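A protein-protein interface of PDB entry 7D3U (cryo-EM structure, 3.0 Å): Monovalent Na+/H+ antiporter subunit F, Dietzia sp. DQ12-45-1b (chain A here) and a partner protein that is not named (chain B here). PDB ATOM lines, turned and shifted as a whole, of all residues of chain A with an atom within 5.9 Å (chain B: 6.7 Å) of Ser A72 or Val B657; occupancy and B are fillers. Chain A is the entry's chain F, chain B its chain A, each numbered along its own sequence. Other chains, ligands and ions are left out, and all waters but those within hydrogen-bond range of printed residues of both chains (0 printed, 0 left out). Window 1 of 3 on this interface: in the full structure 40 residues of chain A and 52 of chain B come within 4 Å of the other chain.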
ATOM      1  N   PHE A  39     -25.400   0.527 -38.479  1.00  0.00           N
ATOM      2  CA  PHE A  39     -25.048  -0.863 -38.203  1.00  0.00           C
ATOM      3  C   PHE A  39     -24.830  -1.628 -39.499  1.00  0.00           C
ATOM      4  O   PHE A  39     -23.880  -2.413 -39.622  1.00  0.00           O
ATOM      5  CB  PHE A  39     -26.135  -1.538 -37.367  1.00  0.00           C
ATOM      6  CG  PHE A  39     -26.366  -0.895 -36.033  1.00  0.00           C
ATOM      7  CD1 PHE A  39     -25.344  -0.232 -35.379  1.00  0.00           C
ATOM      8  CD2 PHE A  39     -27.610  -0.954 -35.430  1.00  0.00           C
ATOM      9  CE1 PHE A  39     -25.559   0.361 -34.152  1.00  0.00           C
ATOM     10  CE2 PHE A  39     -27.830  -0.361 -34.205  1.00  0.00           C
ATOM     11  CZ  PHE A  39     -26.804   0.296 -33.565  1.00  0.00           C
ATOM     12  N   LEU A  67     -27.183 -10.838 -36.968  1.00  0.00           N
ATOM     13  CA  LEU A  67     -27.935 -11.174 -35.766  1.00  0.00           C
ATOM     14  C   LEU A  67     -27.696 -10.185 -34.639  1.00  0.00           C
ATOM     15  O   LEU A  67     -28.288 -10.338 -33.567  1.00  0.00           O
ATOM     16  CB  LEU A  67     -27.575 -12.581 -35.292  1.00  0.00           C
ATOM     17  CG  LEU A  67     -27.694 -13.693 -36.330  1.00  0.00           C
ATOM     18  CD1 LEU A  67     -27.548 -15.047 -35.665  1.00  0.00           C
ATOM     19  CD2 LEU A  67     -29.020 -13.594 -37.056  1.00  0.00           C
ATOM     20  N   VAL A  68     -26.842  -9.189 -34.856  1.00  0.00           N
ATOM     21  CA  VAL A  68     -26.562  -8.163 -33.870  1.00  0.00           C
ATOM     22  C   VAL A  68     -27.098  -6.806 -34.309  1.00  0.00           C
ATOM     23  O   VAL A  68     -27.705  -6.088 -33.513  1.00  0.00           O
ATOM     24  CB  VAL A  68     -25.049  -8.093 -33.577  1.00  0.00           C
ATOM     25  CG1 VAL A  68     -24.680  -6.757 -32.976  1.00  0.00           C
ATOM     26  CG2 VAL A  68     -24.640  -9.225 -32.654  1.00  0.00           C
ATOM     27  N   GLY A  69     -26.903  -6.448 -35.577  1.00  0.00           N
ATOM     28  CA  GLY A  69     -27.507  -5.240 -36.109  1.00  0.00           C
ATOM     29  C   GLY A  69     -29.017  -5.288 -36.203  1.00  0.00           C
ATOM     30  O   GLY A  69     -29.629  -4.282 -36.576  1.00  0.00           O
ATOM     31  N   LEU A  70     -29.625  -6.428 -35.883  1.00  0.00           N
ATOM     32  CA  LEU A  70     -31.073  -6.576 -35.833  1.00  0.00           C
ATOM     33  C   LEU A  70     -31.607  -6.514 -34.408  1.00  0.00           C
ATOM     34  O   LEU A  70     -32.529  -5.745 -34.124  1.00  0.00           O
ATOM     35  CB  LEU A  70     -31.490  -7.896 -36.486  1.00  0.00           C
ATOM     36  CG  LEU A  70     -32.919  -8.348 -36.193  1.00  0.00           C
ATOM     37  CD1 LEU A  70     -33.910  -7.526 -36.995  1.00  0.00           C
ATOM     38  CD2 LEU A  70     -33.078  -9.821 -36.494  1.00  0.00           C
ATOM     39  N   VAL A  71     -31.042  -7.318 -33.503  1.00  0.00           N
ATOM     40  CA  VAL A  71     -31.449  -7.269 -32.103  1.00  0.00           C
ATOM     41  C   VAL A  71     -31.169  -5.896 -31.512  1.00  0.00           C
ATOM     42  O   VAL A  71     -31.933  -5.403 -30.675  1.00  0.00           O
ATOM     43  CB  VAL A  71     -30.744  -8.380 -31.306  1.00  0.00           C
ATOM     44  CG1 VAL A  71     -31.193  -8.362 -29.859  1.00  0.00           C
ATOM     45  CG2 VAL A  71     -31.025  -9.729 -31.931  1.00  0.00           C
ATOM     46  N   SER A  72     -30.087  -5.252 -31.941  1.00  0.00           N
ATOM     47  CA  SER A  72     -29.783  -3.902 -31.488  1.00  0.00           C
ATOM     48  C   SER A  72     -30.549  -2.837 -32.260  1.00  0.00           C
ATOM     49  O   SER A  72     -30.351  -1.647 -31.999  1.00  0.00           O
ATOM     50  CB  SER A  72     -28.282  -3.635 -31.593  1.00  0.00           C
ATOM     51  OG  SER A  72     -27.939  -3.198 -32.893  1.00  0.00           O
ATOM     52  N   ALA A  73     -31.406  -3.230 -33.200  1.00  0.00           N
ATOM     53  CA  ALA A  73     -32.301  -2.304 -33.879  1.00  0.00           C
ATOM     54  C   ALA A  73     -33.734  -2.439 -33.384  1.00  0.00           C
ATOM     55  O   ALA A  73     -34.358  -1.439 -33.019  1.00  0.00           O
ATOM     56  CB  ALA A  73     -32.247  -2.526 -35.394  1.00  0.00           C
ATOM     57  N   LEU A  74     -34.258  -3.667 -33.358  1.00  0.00           N
ATOM     58  CA  LEU A  74     -35.578  -3.914 -32.785  1.00  0.00           C
ATOM     59  C   LEU A  74     -35.683  -3.328 -31.385  1.00  0.00           C
ATOM     60  O   LEU A  74     -36.670  -2.663 -31.047  1.00  0.00           O
ATOM     61  CB  LEU A  74     -35.861  -5.415 -32.754  1.00  0.00           C
ATOM     62  CG  LEU A  74     -35.804  -6.161 -34.084  1.00  0.00           C
ATOM     63  CD1 LEU A  74     -36.043  -7.640 -33.864  1.00  0.00           C
ATOM     64  CD2 LEU A  74     -36.815  -5.594 -35.057  1.00  0.00           C
ATOM     65  N   SER A  75     -34.658  -3.554 -30.560  1.00  0.00           N
ATOM     66  CA  SER A  75     -34.659  -3.012 -29.206  1.00  0.00           C
ATOM     67  C   SER A  75     -34.798  -1.497 -29.223  1.00  0.00           C
ATOM     68  O   SER A  75     -35.522  -0.926 -28.399  1.00  0.00           O
ATOM     69  CB  SER A  75     -33.387  -3.427 -28.473  1.00  0.00           C
ATOM     70  OG  SER A  75     -32.265  -2.721 -28.967  1.00  0.00           O
ATOM     71  N   LEU A  76     -34.125  -0.828 -30.165  1.00  0.00           N
ATOM     72  CA  LEU A  76     -34.287   0.616 -30.285  1.00  0.00           C
ATOM     73  C   LEU A  76     -35.744   0.976 -30.528  1.00  0.00           C
ATOM     74  O   LEU A  76     -36.271   1.912 -29.915  1.00  0.00           O
ATOM     75  CB  LEU A  76     -33.404   1.157 -31.407  1.00  0.00           C
ATOM     76  CG  LEU A  76     -31.900   1.131 -31.143  1.00  0.00           C
ATOM     77  CD1 LEU A  76     -31.171   1.992 -32.156  1.00  0.00           C
ATOM     78  CD2 LEU A  76     -31.600   1.593 -29.730  1.00  0.00           C
ATOM     79  N   ALA B 627     -28.111   4.479 -28.923  1.00  0.00           N
ATOM     80  CA  ALA B 627     -27.763   4.241 -30.320  1.00  0.00           C
ATOM     81  C   ALA B 627     -26.280   4.495 -30.559  1.00  0.00           C
ATOM     82  O   ALA B 627     -25.608   3.718 -31.248  1.00  0.00           O
ATOM     83  CB  ALA B 627     -28.618   5.117 -31.231  1.00  0.00           C
ATOM     84  N   GLY B 630     -24.309   1.569 -29.157  1.00  0.00           N
ATOM     85  CA  GLY B 630     -24.249   0.492 -30.133  1.00  0.00           C
ATOM     86  C   GLY B 630     -23.282   0.792 -31.263  1.00  0.00           C
ATOM     87  O   GLY B 630     -22.561  -0.094 -31.732  1.00  0.00           O
ATOM     88  N   PHE B 634     -19.927  -1.247 -32.303  1.00  0.00           N
ATOM     89  CA  PHE B 634     -19.638  -1.741 -33.646  1.00  0.00           C
ATOM     90  C   PHE B 634     -18.293  -1.230 -34.146  1.00  0.00           C
ATOM     91  O   PHE B 634     -17.540  -1.972 -34.788  1.00  0.00           O
ATOM     92  CB  PHE B 634     -20.751  -1.334 -34.607  1.00  0.00           C
ATOM     93  CG  PHE B 634     -21.739  -2.422 -34.879  1.00  0.00           C
ATOM     94  CD1 PHE B 634     -22.813  -2.626 -34.034  1.00  0.00           C
ATOM     95  CD2 PHE B 634     -21.593  -3.245 -35.978  1.00  0.00           C
ATOM     96  CE1 PHE B 634     -23.724  -3.625 -34.283  1.00  0.00           C
ATOM     97  CE2 PHE B 634     -22.502  -4.247 -36.232  1.00  0.00           C
ATOM     98  CZ  PHE B 634     -23.568  -4.438 -35.383  1.00  0.00           C
ATOM     99  N   GLN B 652     -16.864  -8.747 -28.931  1.00  0.00           N
ATOM    100  CA  GLN B 652     -17.213  -7.338 -28.804  1.00  0.00           C
ATOM    101  C   GLN B 652     -18.562  -7.045 -29.443  1.00  0.00           C
ATOM    102  O   GLN B 652     -19.383  -6.328 -28.863  1.00  0.00           O
ATOM    103  CB  GLN B 652     -16.124  -6.470 -29.427  1.00  0.00           C
ATOM    104  CG  GLN B 652     -16.451  -4.993 -29.435  1.00  0.00           C
ATOM    105  CD  GLN B 652     -16.901  -4.496 -28.081  1.00  0.00           C
ATOM    106  OE1 GLN B 652     -18.031  -4.040 -27.920  1.00  0.00           O
ATOM    107  NE2 GLN B 652     -16.017  -4.580 -27.096  1.00  0.00           N
ATOM    108  N   LEU B 653     -18.810  -7.587 -30.636  1.00  0.00           N
ATOM    109  CA  LEU B 653     -20.121  -7.442 -31.264  1.00  0.00           C
ATOM    110  C   LEU B 653     -21.222  -7.968 -30.355  1.00  0.00           C
ATOM    111  O   LEU B 653     -22.238  -7.295 -30.119  1.00  0.00           O
ATOM    112  CB  LEU B 653     -20.144  -8.181 -32.601  1.00  0.00           C
ATOM    113  CG  LEU B 653     -19.573  -7.464 -33.819  1.00  0.00           C
ATOM    114  CD1 LEU B 653     -19.641  -8.363 -35.036  1.00  0.00           C
ATOM    115  CD2 LEU B 653     -20.330  -6.176 -34.064  1.00  0.00           C
ATOM    116  N   LEU B 654     -21.035  -9.181 -29.832  1.00  0.00           N
ATOM    117  CA  LEU B 654     -22.086  -9.799 -29.030  1.00  0.00           C
ATOM    118  C   LEU B 654     -22.302  -9.055 -27.717  1.00  0.00           C
ATOM    119  O   LEU B 654     -23.443  -8.885 -27.274  1.00  0.00           O
ATOM    120  CB  LEU B 654     -21.745 -11.263 -28.783  1.00  0.00           C
ATOM    121  CG  LEU B 654     -21.785 -12.100 -30.058  1.00  0.00           C
ATOM    122  CD1 LEU B 654     -21.303 -13.505 -29.792  1.00  0.00           C
ATOM    123  CD2 LEU B 654     -23.195 -12.114 -30.611  1.00  0.00           C
ATOM    124  N   VAL B 655     -21.223  -8.590 -27.086  1.00  0.00           N
ATOM    125  CA  VAL B 655     -21.358  -7.835 -25.848  1.00  0.00           C
ATOM    126  C   VAL B 655     -22.001  -6.484 -26.116  1.00  0.00           C
ATOM    127  O   VAL B 655     -22.773  -5.985 -25.293  1.00  0.00           O
ATOM    128  CB  VAL B 655     -19.984  -7.699 -25.165  1.00  0.00           C
ATOM    129  CG1 VAL B 655     -19.969  -6.535 -24.194  1.00  0.00           C
ATOM    130  CG2 VAL B 655     -19.637  -8.985 -24.448  1.00  0.00           C
ATOM    131  N   GLU B 656     -21.739  -5.890 -27.281  1.00  0.00           N
ATOM    132  CA  GLU B 656     -22.413  -4.646 -27.631  1.00  0.00           C
ATOM    133  C   GLU B 656     -23.912  -4.859 -27.775  1.00  0.00           C
ATOM    134  O   GLU B 656     -24.709  -4.056 -27.277  1.00  0.00           O
ATOM    135  CB  GLU B 656     -21.826  -4.073 -28.919  1.00  0.00           C
ATOM    136  CG  GLU B 656     -22.626  -2.926 -29.508  1.00  0.00           C
ATOM    137  CD  GLU B 656     -23.576  -3.381 -30.595  1.00  0.00           C
ATOM    138  OE1 GLU B 656     -23.669  -4.603 -30.823  1.00  0.00           O
ATOM    139  OE2 GLU B 656     -24.229  -2.520 -31.219  1.00  0.00           O
ATOM    140  N   VAL B 657     -24.322  -5.939 -28.444  1.00  0.00           N
ATOM    141  CA  VAL B 657     -25.758  -6.160 -28.607  1.00  0.00           C
ATOM    142  C   VAL B 657     -26.409  -6.488 -27.264  1.00  0.00           C
ATOM    143  O   VAL B 657     -27.510  -6.009 -26.960  1.00  0.00           O
ATOM    144  CB  VAL B 657     -26.037  -7.238 -29.674  1.00  0.00           C
ATOM    145  CG1 VAL B 657     -26.005  -8.641 -29.096  1.00  0.00           C
ATOM    146  CG2 VAL B 657     -27.375  -6.982 -30.336  1.00  0.00           C
ATOM    147  N   LEU B 658     -25.721  -7.256 -26.415  1.00  0.00           N
ATOM    148  CA  LEU B 658     -26.299  -7.638 -25.135  1.00  0.00           C
ATOM    149  C   LEU B 658     -26.221  -6.534 -24.093  1.00  0.00           C
ATOM    150  O   LEU B 658     -26.889  -6.637 -23.061  1.00  0.00           O
ATOM    151  CB  LEU B 658     -25.623  -8.900 -24.601  1.00  0.00           C
ATOM    152  CG  LEU B 658     -26.050 -10.180 -25.315  1.00  0.00           C
ATOM    153  CD1 LEU B 658     -25.398 -11.386 -24.681  1.00  0.00           C
ATOM    154  CD2 LEU B 658     -27.560 -10.317 -25.294  1.00  0.00           C
ATOM    155  N   THR B 659     -25.424  -5.495 -24.323  1.00  0.00           N
ATOM    156  CA  THR B 659     -25.490  -4.325 -23.464  1.00  0.00           C
ATOM    157  C   THR B 659     -26.468  -3.291 -23.994  1.00  0.00           C
ATOM    158  O   THR B 659     -27.069  -2.563 -23.202  1.00  0.00           O
ATOM    159  CB  THR B 659     -24.100  -3.702 -23.281  1.00  0.00           C
ATOM    160  OG1 THR B 659     -24.123  -2.802 -22.167  1.00  0.00           O
ATOM    161  CG2 THR B 659     -23.664  -2.940 -24.518  1.00  0.00           C
ATOM    162  N   VAL B 660     -26.683  -3.240 -25.311  1.00  0.00           N
ATOM    163  CA  VAL B 660     -27.736  -2.388 -25.850  1.00  0.00           C
ATOM    164  C   VAL B 660     -29.099  -2.888 -25.395  1.00  0.00           C
ATOM    165  O   VAL B 660     -29.972  -2.095 -25.020  1.00  0.00           O
ATOM    166  CB  VAL B 660     -27.634  -2.317 -27.384  1.00  0.00           C
ATOM    167  CG1 VAL B 660     -28.966  -1.920 -27.990  1.00  0.00           C
ATOM    168  CG2 VAL B 660     -26.554  -1.339 -27.793  1.00  0.00           C
ATOM    169  N   VAL B 661     -29.298  -4.208 -25.399  1.00  0.00           N
ATOM    170  CA  VAL B 661     -30.566  -4.765 -24.931  1.00  0.00           C
ATOM    171  C   VAL B 661     -30.814  -4.392 -23.473  1.00  0.00           C
ATOM    172  O   VAL B 661     -31.918  -3.977 -23.099  1.00  0.00           O
ATOM    173  CB  VAL B 661     -30.589  -6.289 -25.139  1.00  0.00           C
ATOM    174  CG1 VAL B 661     -31.757  -6.905 -24.399  1.00  0.00           C
ATOM    175  CG2 VAL B 661     -30.672  -6.614 -26.615  1.00  0.00           C
ATOM    176  N   VAL B 662     -29.787  -4.510 -22.629  1.00  0.00           N
ATOM    177  CA  VAL B 662     -29.968  -4.227 -21.208  1.00  0.00           C
ATOM    178  C   VAL B 662     -30.163  -2.733 -20.973  1.00  0.00           C
ATOM    179  O   VAL B 662     -30.971  -2.325 -20.127  1.00  0.00           O
ATOM    180  CB  VAL B 662     -28.784  -4.785 -20.401  1.00  0.00           C
ATOM    181  CG1 VAL B 662     -28.872  -4.344 -18.954  1.00  0.00           C
ATOM    182  CG2 VAL B 662     -28.764  -6.297 -20.485  1.00  0.00           C
ATOM    183  N   LEU B 825     -22.891 -15.753 -25.734  1.00  0.00           N
ATOM    184  CA  LEU B 825     -23.493 -14.455 -26.002  1.00  0.00           C
ATOM    185  C   LEU B 825     -24.376 -14.497 -27.245  1.00  0.00           C
ATOM    186  O   LEU B 825     -25.364 -13.759 -27.325  1.00  0.00           O
ATOM    187  CB  LEU B 825     -22.409 -13.389 -26.135  1.00  0.00           C
ATOM    188  CG  LEU B 825     -21.461 -13.222 -24.943  1.00  0.00           C
ATOM    189  CD1 LEU B 825     -20.176 -12.537 -25.369  1.00  0.00           C
ATOM    190  CD2 LEU B 825     -22.118 -12.464 -23.806  1.00  0.00           C
ATOM    191  N   GLY B 828     -27.485 -15.662 -25.803  1.00  0.00           N
ATOM    192  CA  GLY B 828     -28.099 -14.533 -25.126  1.00  0.00           C
ATOM    193  C   GLY B 828     -28.812 -13.610 -26.095  1.00  0.00           C
ATOM    194  O   GLY B 828     -29.860 -13.044 -25.775  1.00  0.00           O
ATOM    195  N   ALA B 829     -28.253 -13.444 -27.294  1.00  0.00           N
ATOM    196  CA  ALA B 829     -28.949 -12.694 -28.332  1.00  0.00           C
ATOM    197  C   ALA B 829     -30.253 -13.381 -28.722  1.00  0.00           C
ATOM    198  O   ALA B 829     -31.264 -12.718 -28.975  1.00  0.00           O
ATOM    199  CB  ALA B 829     -28.046 -12.518 -29.552  1.00  0.00           C
ATOM    200  N   ALA B 832     -32.701 -12.559 -26.079  1.00  0.00           N
ATOM    201  CA  ALA B 832     -33.216 -11.212 -26.310  1.00  0.00           C
ATOM    202  C   ALA B 832     -34.256 -11.208 -27.423  1.00  0.00           C
ATOM    203  O   ALA B 832     -35.252 -10.476 -27.351  1.00  0.00           O
ATOM    204  CB  ALA B 832     -32.069 -10.261 -26.641  1.00  0.00           C
ATOM    205  N   LEU B 836     -38.102  -9.917 -27.098  1.00  0.00           N
ATOM    206  CA  LEU B 836     -38.728  -8.943 -27.987  1.00  0.00           C
ATOM    207  C   LEU B 836     -39.914  -9.538 -28.735  1.00  0.00           C
ATOM    208  O   LEU B 836     -40.810  -8.802 -29.165  1.00  0.00           O
ATOM    209  CB  LEU B 836     -37.701  -8.404 -28.982  1.00  0.00           C
ATOM    210  CG  LEU B 836     -36.490  -7.670 -28.409  1.00  0.00           C
ATOM    211  CD1 LEU B 836     -35.535  -7.286 -29.521  1.00  0.00           C
ATOM    212  CD2 LEU B 836     -36.928  -6.444 -27.635  1.00  0.00           C
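Of the printed residues of chain B, Val A68 touches Phe B634, Leu B653, Leu B654, Glu B656 and Val B657. Leu A70 touches none of the printed residues of chain B. Of the printed residues of chain B, Val A71 touches Val B657 (3.8 Å), Val B661 (3.7 Å) and Ala B832 (3.8 Å). Printed residues of chain B within 4 Å of Ser A72: Val B657 (3.6 Å). Of the printed residues of chain A, Leu B654 touches Val A68. Of chain A, only Val A68 (3.3 Å), Val A71 (3.8 Å) and Ser A72 (3.6 Å) come within 4 Å of Val B657. Thr B659 touches none of the printed residues of chain A. The nearest printed residue of chain A that does not touch Leu B653 is Gly A69 (6.8 Å).
Of the 19 printed residues of chain B, 10 touch a printed residue of chain A. Printed residues of chain B that touch a printed residue of chain A: Gly B630, Phe B634, Leu B653, Leu B654, Glu B656, Val B657, Val B660, Val B661, Ala B832 and Leu B836. Along chain B the printed residues that touch a printed residue of chain A span positions 630 to 836. Of the 11 printed residues of chain A, 7 touch a printed residue of chain B. Hydrophobic or aromatic side chains of chain A within 4 Å of the printed part of chain B: Phe A39, Val A68, Val A71 and Leu A74. Among the printed residues, no Asp or Glu carboxylate lies within 4 Å of a Lys or Arg side-chain nitrogen of the other chain.
Phe A39 touches Gly B630 (CE1 to C, 3.7 Å). Phe B634 touches Phe A39 (CD1 to CD1, 3.7 Å). CZ of Phe B634 touches CG1 of Val A68, 3.5 Å away. Leu B654 touches Val A68 (CD2 to CG2, 3.8 Å). CG1 of Val A68 touches OE1 of Glu B656, 3.2 Å away. Val A71 touches Val B657. CG1 of Val A71 touches CG2 of Val B661, at 3.7 Å. Val A71 touches Ala B832 (CG1 to CB, 3.8 Å). Ser A72 touches Val B657. Leu B836 touches Ser A75.
The backbone carbonyl oxygen of Val A68 lies within hydrogen-bond range of the side-chain hydroxyl of Ser A72 (3.0 Å). The backbone carbonyl oxygen of Val A71 is in hydrogen-bond range of the side-chain hydroxyl of Ser A75, 3.2 Å away.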
